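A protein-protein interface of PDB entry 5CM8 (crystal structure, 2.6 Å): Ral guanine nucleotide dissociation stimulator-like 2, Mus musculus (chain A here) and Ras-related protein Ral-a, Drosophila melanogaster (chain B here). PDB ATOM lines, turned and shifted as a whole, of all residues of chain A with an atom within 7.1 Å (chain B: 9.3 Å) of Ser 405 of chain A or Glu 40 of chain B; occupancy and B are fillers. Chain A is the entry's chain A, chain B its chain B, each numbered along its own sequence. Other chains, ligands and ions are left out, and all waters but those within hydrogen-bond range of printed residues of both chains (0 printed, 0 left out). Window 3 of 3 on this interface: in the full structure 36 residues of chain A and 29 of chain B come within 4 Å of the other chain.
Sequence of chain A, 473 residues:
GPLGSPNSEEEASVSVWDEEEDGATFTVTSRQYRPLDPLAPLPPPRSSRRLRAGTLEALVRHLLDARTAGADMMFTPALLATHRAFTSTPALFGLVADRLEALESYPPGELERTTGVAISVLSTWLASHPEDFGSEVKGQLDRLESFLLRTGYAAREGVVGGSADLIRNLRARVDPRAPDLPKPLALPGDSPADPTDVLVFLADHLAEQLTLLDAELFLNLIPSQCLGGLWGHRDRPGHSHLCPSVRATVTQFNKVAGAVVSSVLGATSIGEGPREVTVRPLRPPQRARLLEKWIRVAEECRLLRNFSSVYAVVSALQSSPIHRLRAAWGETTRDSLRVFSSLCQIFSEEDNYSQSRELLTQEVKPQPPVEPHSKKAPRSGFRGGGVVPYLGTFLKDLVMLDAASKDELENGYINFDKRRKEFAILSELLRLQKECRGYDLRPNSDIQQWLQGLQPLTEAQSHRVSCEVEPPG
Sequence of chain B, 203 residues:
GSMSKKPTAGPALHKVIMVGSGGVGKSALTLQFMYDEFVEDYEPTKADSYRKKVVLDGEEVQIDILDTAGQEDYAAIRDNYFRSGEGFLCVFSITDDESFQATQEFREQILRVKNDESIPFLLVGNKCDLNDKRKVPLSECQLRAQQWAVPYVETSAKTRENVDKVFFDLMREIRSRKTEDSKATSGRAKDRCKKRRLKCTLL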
ATOM      1  N   MET A 400     -32.933  -4.421 -31.348  1.00  0.00           N
ATOM      2  CA  MET A 400     -31.755  -5.172 -30.953  1.00  0.00           C
ATOM      3  C   MET A 400     -31.148  -4.563 -29.699  1.00  0.00           C
ATOM      4  O   MET A 400     -30.744  -5.281 -28.777  1.00  0.00           O
ATOM      5  CB  MET A 400     -30.726  -5.166 -32.083  1.00  0.00           C
ATOM      6  CG  MET A 400     -29.877  -6.421 -32.162  1.00  0.00           C
ATOM      7  SD  MET A 400     -30.810  -7.911 -32.573  1.00  0.00           S
ATOM      8  CE  MET A 400     -31.217  -7.620 -34.295  1.00  0.00           C
ATOM      9  N   LEU A 401     -31.106  -3.233 -29.673  1.00  0.00           N
ATOM     10  CA  LEU A 401     -30.510  -2.479 -28.578  1.00  0.00           C
ATOM     11  C   LEU A 401     -31.368  -2.583 -27.323  1.00  0.00           C
ATOM     12  O   LEU A 401     -30.848  -2.585 -26.210  1.00  0.00           O
ATOM     13  CB  LEU A 401     -30.339  -1.018 -28.995  1.00  0.00           C
ATOM     14  CG  LEU A 401     -29.119  -0.199 -28.568  1.00  0.00           C
ATOM     15  CD1 LEU A 401     -27.800  -0.930 -28.769  1.00  0.00           C
ATOM     16  CD2 LEU A 401     -29.115   1.085 -29.357  1.00  0.00           C
ATOM     17  N   ASP A 402     -32.681  -2.689 -27.517  1.00  0.00           N
ATOM     18  CA  ASP A 402     -33.625  -2.880 -26.416  1.00  0.00           C
ATOM     19  C   ASP A 402     -33.400  -4.198 -25.671  1.00  0.00           C
ATOM     20  O   ASP A 402     -33.619  -4.277 -24.463  1.00  0.00           O
ATOM     21  CB  ASP A 402     -35.063  -2.816 -26.927  1.00  0.00           C
ATOM     22  CG  ASP A 402     -36.088  -2.909 -25.810  1.00  0.00           C
ATOM     23  OD1 ASP A 402     -35.959  -2.162 -24.820  1.00  0.00           O
ATOM     24  OD2 ASP A 402     -37.024  -3.732 -25.924  1.00  0.00           O
ATOM     25  N   ALA A 403     -32.971  -5.228 -26.399  1.00  0.00           N
ATOM     26  CA  ALA A 403     -32.742  -6.548 -25.821  1.00  0.00           C
ATOM     27  C   ALA A 403     -31.338  -6.697 -25.232  1.00  0.00           C
ATOM     28  O   ALA A 403     -31.095  -7.591 -24.421  1.00  0.00           O
ATOM     29  CB  ALA A 403     -33.008  -7.632 -26.858  1.00  0.00           C
ATOM     30  N   ALA A 404     -30.422  -5.819 -25.635  1.00  0.00           N
ATOM     31  CA  ALA A 404     -29.039  -5.867 -25.153  1.00  0.00           C
ATOM     32  C   ALA A 404     -28.889  -5.380 -23.709  1.00  0.00           C
ATOM     33  O   ALA A 404     -27.932  -5.738 -23.029  1.00  0.00           O
ATOM     34  CB  ALA A 404     -28.123  -5.076 -26.079  1.00  0.00           C
ATOM     35  N   SER A 405     -29.832  -4.562 -23.250  1.00  0.00           N
ATOM     36  CA  SER A 405     -29.769  -3.995 -21.906  1.00  0.00           C
ATOM     37  C   SER A 405     -31.118  -4.056 -21.203  1.00  0.00           C
ATOM     38  O   SER A 405     -32.171  -3.986 -21.842  1.00  0.00           O
ATOM     39  CB  SER A 405     -29.293  -2.540 -21.956  1.00  0.00           C
ATOM     40  OG  SER A 405     -28.117  -2.395 -22.728  1.00  0.00           O
ATOM     41  N   LYS A 406     -31.077  -4.193 -19.883  1.00  0.00           N
ATOM     42  CA  LYS A 406     -32.269  -4.033 -19.065  1.00  0.00           C
ATOM     43  C   LYS A 406     -32.491  -2.544 -18.832  1.00  0.00           C
ATOM     44  O   LYS A 406     -31.532  -1.769 -18.745  1.00  0.00           O
ATOM     45  CB  LYS A 406     -32.122  -4.776 -17.734  1.00  0.00           C
ATOM     46  CG  LYS A 406     -32.242  -6.290 -17.855  1.00  0.00           C
ATOM     47  CD  LYS A 406     -31.744  -6.994 -16.605  1.00  0.00           C
ATOM     48  CE  LYS A 406     -31.510  -8.479 -16.866  1.00  0.00           C
ATOM     49  NZ  LYS A 406     -30.689  -9.117 -15.795  1.00  0.00           N
ATOM     50  N   ASP A 407     -33.756  -2.146 -18.754  1.00  0.00           N
ATOM     51  CA  ASP A 407     -34.108  -0.755 -18.486  1.00  0.00           C
ATOM     52  C   ASP A 407     -33.544  -0.312 -17.138  1.00  0.00           C
ATOM     53  O   ASP A 407     -33.021   0.796 -17.010  1.00  0.00           O
ATOM     54  CB  ASP A 407     -35.630  -0.564 -18.500  1.00  0.00           C
ATOM     55  CG  ASP A 407     -36.254  -0.869 -19.849  1.00  0.00           C
ATOM     56  OD1 ASP A 407     -35.553  -0.796 -20.879  1.00  0.00           O
ATOM     57  OD2 ASP A 407     -37.466  -1.172 -19.881  1.00  0.00           O
ATOM     58  N   GLU A 408     -33.642  -1.201 -16.150  1.00  0.00           N
ATOM     59  CA  GLU A 408     -33.261  -0.909 -14.773  1.00  0.00           C
ATOM     60  C   GLU A 408     -32.061  -1.739 -14.325  1.00  0.00           C
ATOM     61  O   GLU A 408     -31.857  -2.857 -14.801  1.00  0.00           O
ATOM     62  CB  GLU A 408     -34.436  -1.174 -13.822  1.00  0.00           C
ATOM     63  CG  GLU A 408     -35.776  -0.550 -14.235  1.00  0.00           C
ATOM     64  CD  GLU A 408     -36.607  -1.441 -15.162  1.00  0.00           C
ATOM     65  OE1 GLU A 408     -36.390  -2.673 -15.192  1.00  0.00           O
ATOM     66  OE2 GLU A 408     -37.491  -0.900 -15.863  1.00  0.00           O
ATOM     67  N   LEU A 409     -31.268  -1.181 -13.411  1.00  0.00           N
ATOM     68  CA  LEU A 409     -30.229  -1.947 -12.728  1.00  0.00           C
ATOM     69  C   LEU A 409     -30.848  -2.690 -11.550  1.00  0.00           C
ATOM     70  O   LEU A 409     -31.998  -2.428 -11.179  1.00  0.00           O
ATOM     71  CB  LEU A 409     -29.096  -1.038 -12.237  1.00  0.00           C
ATOM     72  CG  LEU A 409     -28.165  -0.336 -13.230  1.00  0.00           C
ATOM     73  CD1 LEU A 409     -27.062   0.386 -12.472  1.00  0.00           C
ATOM     74  CD2 LEU A 409     -27.557  -1.306 -14.236  1.00  0.00           C
ATOM     75  N   ASN A 415     -31.201   2.639 -15.953  1.00  0.00           N
ATOM     76  CA  ASN A 415     -29.961   2.382 -16.675  1.00  0.00           C
ATOM     77  C   ASN A 415     -29.842   3.348 -17.846  1.00  0.00           C
ATOM     78  O   ASN A 415     -30.331   3.068 -18.945  1.00  0.00           O
ATOM     79  CB  ASN A 415     -29.924   0.922 -17.150  1.00  0.00           C
ATOM     80  CG  ASN A 415     -28.673   0.578 -17.950  1.00  0.00           C
ATOM     81  OD1 ASN A 415     -27.609   1.177 -17.773  1.00  0.00           O
ATOM     82  ND2 ASN A 415     -28.798  -0.410 -18.829  1.00  0.00           N
ATOM     83  N   ASP A 417     -27.207   4.206 -19.474  1.00  0.00           N
ATOM     84  CA  ASP A 417     -26.309   3.655 -20.500  1.00  0.00           C
ATOM     85  C   ASP A 417     -27.091   3.247 -21.753  1.00  0.00           C
ATOM     86  O   ASP A 417     -26.725   3.613 -22.871  1.00  0.00           O
ATOM     87  CB  ASP A 417     -25.544   2.438 -19.961  1.00  0.00           C
ATOM     88  CG  ASP A 417     -24.402   2.820 -19.029  1.00  0.00           C
ATOM     89  OD1 ASP A 417     -23.555   3.657 -19.416  1.00  0.00           O
ATOM     90  OD2 ASP A 417     -24.342   2.258 -17.910  1.00  0.00           O
ATOM     91  N   LYS A 418     -28.171   2.498 -21.540  1.00  0.00           N
ATOM     92  CA  LYS A 418     -29.067   2.050 -22.600  1.00  0.00           C
ATOM     93  C   LYS A 418     -29.643   3.228 -23.385  1.00  0.00           C
ATOM     94  O   LYS A 418     -29.692   3.202 -24.614  1.00  0.00           O
ATOM     95  CB  LYS A 418     -30.203   1.226 -21.995  1.00  0.00           C
ATOM     96  CG  LYS A 418     -31.083   0.528 -23.009  1.00  0.00           C
ATOM     97  CD  LYS A 418     -32.192  -0.244 -22.330  1.00  0.00           C
ATOM     98  CE  LYS A 418     -32.936  -1.081 -23.343  1.00  0.00           C
ATOM     99  NZ  LYS A 418     -34.116  -1.765 -22.756  1.00  0.00           N
ATOM    100  N   ARG A 419     -30.056   4.262 -22.661  1.00  0.00           N
ATOM    101  CA  ARG A 419     -30.699   5.424 -23.259  1.00  0.00           C
ATOM    102  C   ARG A 419     -29.755   6.216 -24.158  1.00  0.00           C
ATOM    103  O   ARG A 419     -30.170   6.711 -25.202  1.00  0.00           O
ATOM    104  CB  ARG A 419     -31.319   6.314 -22.177  1.00  0.00           C
ATOM    105  CG  ARG A 419     -32.236   5.570 -21.198  1.00  0.00           C
ATOM    106  CD  ARG A 419     -33.358   4.801 -21.900  1.00  0.00           C
ATOM    107  NE  ARG A 419     -34.146   4.007 -20.958  1.00  0.00           N
ATOM    108  CZ  ARG A 419     -35.042   3.082 -21.304  1.00  0.00           C
ATOM    109  NH1 ARG A 419     -35.276   2.807 -22.584  1.00  0.00           N
ATOM    110  NH2 ARG A 419     -35.703   2.421 -20.363  1.00  0.00           N
ATOM    111  N   LYS A 421     -27.204   4.894 -25.852  1.00  0.00           N
ATOM    112  CA  LYS A 421     -27.028   4.075 -27.049  1.00  0.00           C
ATOM    113  C   LYS A 421     -28.229   4.206 -27.983  1.00  0.00           C
ATOM    114  O   LYS A 421     -28.067   4.288 -29.203  1.00  0.00           O
ATOM    115  CB  LYS A 421     -26.808   2.607 -26.673  1.00  0.00           C
ATOM    116  CG  LYS A 421     -25.428   2.315 -26.094  1.00  0.00           C
ATOM    117  CD  LYS A 421     -25.405   1.000 -25.330  1.00  0.00           C
ATOM    118  CE  LYS A 421     -24.028   0.748 -24.741  1.00  0.00           C
ATOM    119  NZ  LYS A 421     -23.980  -0.519 -23.960  1.00  0.00           N
ATOM    120  N   ALA B  28     -33.014 -11.670 -28.745  1.00  0.00           N
ATOM    121  CA  ALA B  28     -32.372 -12.195 -27.542  1.00  0.00           C
ATOM    122  C   ALA B  28     -31.529 -13.439 -27.826  1.00  0.00           C
ATOM    123  O   ALA B  28     -30.517 -13.671 -27.165  1.00  0.00           O
ATOM    124  CB  ALA B  28     -33.413 -12.481 -26.468  1.00  0.00           C
ATOM    125  N   LEU B  31     -28.134 -12.219 -29.782  1.00  0.00           N
ATOM    126  CA  LEU B  31     -27.232 -11.503 -28.887  1.00  0.00           C
ATOM    127  C   LEU B  31     -26.569 -12.437 -27.887  1.00  0.00           C
ATOM    128  O   LEU B  31     -25.366 -12.337 -27.643  1.00  0.00           O
ATOM    129  CB  LEU B  31     -27.984 -10.392 -28.146  1.00  0.00           C
ATOM    130  CG  LEU B  31     -28.505  -9.206 -28.960  1.00  0.00           C
ATOM    131  CD1 LEU B  31     -29.534  -8.436 -28.155  1.00  0.00           C
ATOM    132  CD2 LEU B  31     -27.369  -8.292 -29.404  1.00  0.00           C
ATOM    133  N   GLN B  32     -27.356 -13.345 -27.315  1.00  0.00           N
ATOM    134  CA  GLN B  32     -26.845 -14.287 -26.328  1.00  0.00           C
ATOM    135  C   GLN B  32     -25.867 -15.278 -26.955  1.00  0.00           C
ATOM    136  O   GLN B  32     -24.897 -15.687 -26.311  1.00  0.00           O
ATOM    137  CB  GLN B  32     -27.995 -15.014 -25.623  1.00  0.00           C
ATOM    138  CG  GLN B  32     -27.605 -15.721 -24.323  1.00  0.00           C
ATOM    139  CD  GLN B  32     -26.958 -14.795 -23.301  1.00  0.00           C
ATOM    140  OE1 GLN B  32     -27.445 -13.691 -23.043  1.00  0.00           O
ATOM    141  NE2 GLN B  32     -25.857 -15.247 -22.712  1.00  0.00           N
ATOM    142  N   TYR B  35     -22.660 -12.828 -28.317  1.00  0.00           N
ATOM    143  CA  TYR B  35     -21.990 -12.146 -27.215  1.00  0.00           C
ATOM    144  C   TYR B  35     -22.253 -12.886 -25.908  1.00  0.00           C
ATOM    145  O   TYR B  35     -23.397 -13.223 -25.590  1.00  0.00           O
ATOM    146  CB  TYR B  35     -22.459 -10.689 -27.122  1.00  0.00           C
ATOM    147  CG  TYR B  35     -22.299  -9.902 -28.408  1.00  0.00           C
ATOM    148  CD1 TYR B  35     -23.277  -9.944 -29.402  1.00  0.00           C
ATOM    149  CD2 TYR B  35     -21.172  -9.113 -28.629  1.00  0.00           C
ATOM    150  CE1 TYR B  35     -23.134  -9.227 -30.585  1.00  0.00           C
ATOM    151  CE2 TYR B  35     -21.020  -8.390 -29.808  1.00  0.00           C
ATOM    152  CZ  TYR B  35     -22.004  -8.451 -30.781  1.00  0.00           C
ATOM    153  OH  TYR B  35     -21.859  -7.738 -31.949  1.00  0.00           O
ATOM    154  N   ASP B  36     -21.187 -13.141 -25.156  1.00  0.00           N
ATOM    155  CA  ASP B  36     -21.279 -13.938 -23.935  1.00  0.00           C
ATOM    156  C   ASP B  36     -21.320 -13.055 -22.681  1.00  0.00           C
ATOM    157  O   ASP B  36     -22.395 -12.614 -22.262  1.00  0.00           O
ATOM    158  CB  ASP B  36     -20.121 -14.948 -23.870  1.00  0.00           C
ATOM    159  CG  ASP B  36     -20.490 -16.233 -23.138  1.00  0.00           C
ATOM    160  OD1 ASP B  36     -21.487 -16.246 -22.379  1.00  0.00           O
ATOM    161  OD2 ASP B  36     -19.772 -17.238 -23.325  1.00  0.00           O
ATOM    162  N   GLU B  37     -20.149 -12.800 -22.097  1.00  0.00           N
ATOM    163  CA  GLU B  37     -20.029 -11.995 -20.881  1.00  0.00           C
ATOM    164  C   GLU B  37     -19.992 -10.496 -21.188  1.00  0.00           C
ATOM    165  O   GLU B  37     -20.158  -9.666 -20.286  1.00  0.00           O
ATOM    166  CB  GLU B  37     -18.791 -12.410 -20.091  1.00  0.00           C
ATOM    167  N   PHE B  38     -19.778 -10.165 -22.460  1.00  0.00           N
ATOM    168  CA  PHE B  38     -19.690  -8.776 -22.916  1.00  0.00           C
ATOM    169  C   PHE B  38     -20.792  -8.437 -23.927  1.00  0.00           C
ATOM    170  O   PHE B  38     -20.522  -7.956 -25.033  1.00  0.00           O
ATOM    171  CB  PHE B  38     -18.287  -8.465 -23.469  1.00  0.00           C
ATOM    172  CG  PHE B  38     -17.454  -9.690 -23.759  1.00  0.00           C
ATOM    173  CD1 PHE B  38     -17.555 -10.347 -24.984  1.00  0.00           C
ATOM    174  CD2 PHE B  38     -16.566 -10.184 -22.804  1.00  0.00           C
ATOM    175  CE1 PHE B  38     -16.785 -11.482 -25.253  1.00  0.00           C
ATOM    176  CE2 PHE B  38     -15.793 -11.318 -23.061  1.00  0.00           C
ATOM    177  CZ  PHE B  38     -15.902 -11.967 -24.288  1.00  0.00           C
ATOM    178  N   VAL B  39     -22.034  -8.694 -23.520  1.00  0.00           N
ATOM    179  CA  VAL B  39     -23.221  -8.399 -24.325  1.00  0.00           C
ATOM    180  C   VAL B  39     -23.506  -6.892 -24.366  1.00  0.00           C
ATOM    181  O   VAL B  39     -24.094  -6.390 -25.327  1.00  0.00           O
ATOM    182  CB  VAL B  39     -24.470  -9.212 -23.834  1.00  0.00           C
ATOM    183  CG1 VAL B  39     -24.854  -8.847 -22.399  1.00  0.00           C
ATOM    184  CG2 VAL B  39     -25.658  -9.037 -24.776  1.00  0.00           C
ATOM    185  N   GLU B  40     -23.067  -6.185 -23.327  1.00  0.00           N
ATOM    186  CA  GLU B  40     -23.270  -4.740 -23.212  1.00  0.00           C
ATOM    187  C   GLU B  40     -22.504  -3.967 -24.285  1.00  0.00           C
ATOM    188  O   GLU B  40     -22.997  -2.964 -24.801  1.00  0.00           O
ATOM    189  CB  GLU B  40     -22.883  -4.245 -21.811  1.00  0.00           C
ATOM    190  CG  GLU B  40     -23.728  -4.820 -20.666  1.00  0.00           C
ATOM    191  CD  GLU B  40     -25.088  -4.144 -20.510  1.00  0.00           C
ATOM    192  OE1 GLU B  40     -25.873  -4.118 -21.485  1.00  0.00           O
ATOM    193  OE2 GLU B  40     -25.377  -3.648 -19.397  1.00  0.00           O
ATOM    194  N   ASP B  41     -21.305  -4.446 -24.619  1.00  0.00           N
ATOM    195  CA  ASP B  41     -20.504  -3.859 -25.692  1.00  0.00           C
ATOM    196  C   ASP B  41     -20.981  -4.303 -27.078  1.00  0.00           C
ATOM    197  O   ASP B  41     -20.192  -4.792 -27.896  1.00  0.00           O
ATOM    198  CB  ASP B  41     -19.018  -4.186 -25.501  1.00  0.00           C
ATOM    199  CG  ASP B  41     -18.255  -3.071 -24.805  1.00  0.00           C
ATOM    200  OD1 ASP B  41     -18.170  -1.956 -25.367  1.00  0.00           O
ATOM    201  OD2 ASP B  41     -17.723  -3.315 -23.702  1.00  0.00           O
ATOM    202  N   TYR B  42     -22.276  -4.131 -27.335  1.00  0.00           N
ATOM    203  CA  TYR B  42     -22.852  -4.425 -28.643  1.00  0.00           C
ATOM    204  C   TYR B  42     -23.122  -3.138 -29.415  1.00  0.00           C
ATOM    205  O   TYR B  42     -23.878  -2.279 -28.955  1.00  0.00           O
ATOM    206  CB  TYR B  42     -24.138  -5.250 -28.508  1.00  0.00           C
ATOM    207  CG  TYR B  42     -24.991  -5.260 -29.760  1.00  0.00           C
ATOM    208  CD1 TYR B  42     -24.611  -5.999 -30.879  1.00  0.00           C
ATOM    209  CD2 TYR B  42     -26.172  -4.521 -29.829  1.00  0.00           C
ATOM    210  CE1 TYR B  42     -25.385  -6.006 -32.034  1.00  0.00           C
ATOM    211  CE2 TYR B  42     -26.952  -4.521 -30.980  1.00  0.00           C
ATOM    212  CZ  TYR B  42     -26.554  -5.266 -32.077  1.00  0.00           C
ATOM    213  OH  TYR B  42     -27.318  -5.270 -33.219  1.00  0.00           O
ATOM    214  N   GLU B  43     -22.495  -3.014 -30.582  1.00  0.00           N
ATOM    215  CA  GLU B  43     -22.721  -1.887 -31.482  1.00  0.00           C
ATOM    216  C   GLU B  43     -23.541  -2.327 -32.702  1.00  0.00           C
ATOM    217  O   GLU B  43     -23.039  -3.066 -33.552  1.00  0.00           O
ATOM    218  CB  GLU B  43     -21.393  -1.256 -31.917  1.00  0.00           C
ATOM    219  CG  GLU B  43     -20.797  -0.267 -30.915  1.00  0.00           C
ATOM    220  CD  GLU B  43     -19.902  -0.925 -29.878  1.00  0.00           C
ATOM    221  OE1 GLU B  43     -18.950  -1.639 -30.271  1.00  0.00           O
ATOM    222  OE2 GLU B  43     -20.136  -0.715 -28.667  1.00  0.00           O
ATOM    223  N   PRO B  44     -24.809  -1.875 -32.785  1.00  0.00           N
ATOM    224  CA  PRO B  44     -25.751  -2.297 -33.833  1.00  0.00           C
ATOM    225  C   PRO B  44     -25.457  -1.835 -35.268  1.00  0.00           C
ATOM    226  O   PRO B  44     -26.088  -2.336 -36.200  1.00  0.00           O
ATOM    227  CB  PRO B  44     -27.086  -1.706 -33.358  1.00  0.00           C
ATOM    228  CG  PRO B  44     -26.710  -0.578 -32.474  1.00  0.00           C
ATOM    229  CD  PRO B  44     -25.471  -1.030 -31.774  1.00  0.00           C
ATOM    230  N   LYS B 158     -33.258 -16.470 -21.369  1.00  0.00           N
ATOM    231  CA  LYS B 158     -32.246 -15.852 -20.503  1.00  0.00           C
ATOM    232  C   LYS B 158     -31.292 -16.837 -19.817  1.00  0.00           C
ATOM    233  O   LYS B 158     -30.220 -16.442 -19.352  1.00  0.00           O
ATOM    234  CB  LYS B 158     -32.919 -14.957 -19.451  1.00  0.00           C
ATOM    235  CG  LYS B 158     -33.774 -13.810 -20.004  1.00  0.00           C
ATOM    236  CD  LYS B 158     -32.972 -12.527 -20.250  1.00  0.00           C
ATOM    237  CE  LYS B 158     -32.734 -12.262 -21.735  1.00  0.00           C
ATOM    238  NZ  LYS B 158     -31.583 -13.021 -22.297  1.00  0.00           N
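The backbone carbonyl oxygen of Ala 404 of chain A lies close to the side-chain carboxylate of Glu 40 of chain B, 3.0 Å away. The side-chain hydroxyl of Ser 405 of chain A lies within hydrogen-bond range of the side-chain carboxylate of Glu 40 of chain B (3.1 Å). The side-chain amino group (NZ) of Lys 421 of chain A sits at hydrogen-bond distance from the backbone carbonyl oxygen (O) of Glu 40 of chain B (2.8 Å).
Of the printed residues of chain B, Ala 403 of chain A touches Leu 31. Lys 406 of chain A touches none of the printed residues of chain B. Printed residues of chain B within 4 Å of Lys 421 of chain A: Glu 40 (2.8 Å). Glu 40 of chain B touches three residues of chain A. Printed residues of chain A within 4 Å of Tyr 42 of chain B: Met 400 (3.0 Å).
The backbone carbonyl oxygen (O) of Ser 405 of chain A is in hydrogen-bond range of the side-chain amino group (NZ) of Lys 418 of chain A (3.1 Å).
Among the printed residues, pairs that only touch across the chains: Met 400 of chain A with Leu 31 of chain B (3.4 Å), Met 400 of chain A with Tyr 42 of chain B (3.0 Å), Leu 401 of chain A with Pro 44 of chain B (3.8 Å), Ala 403 of chain A with Leu 31 of chain B (3.8 Å) and Ala 404 of chain A with Leu 31 of chain B (3.7 Å).
Of the 15 printed residues of chain A, 6 touch a printed residue of chain B. Of the 14 printed residues of chain B, 4 touch a printed residue of chain A. Among the printed residues, no Asp or Glu carboxylate lies within 4 Å of a Lys or Arg side-chain nitrogen of the other chain.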
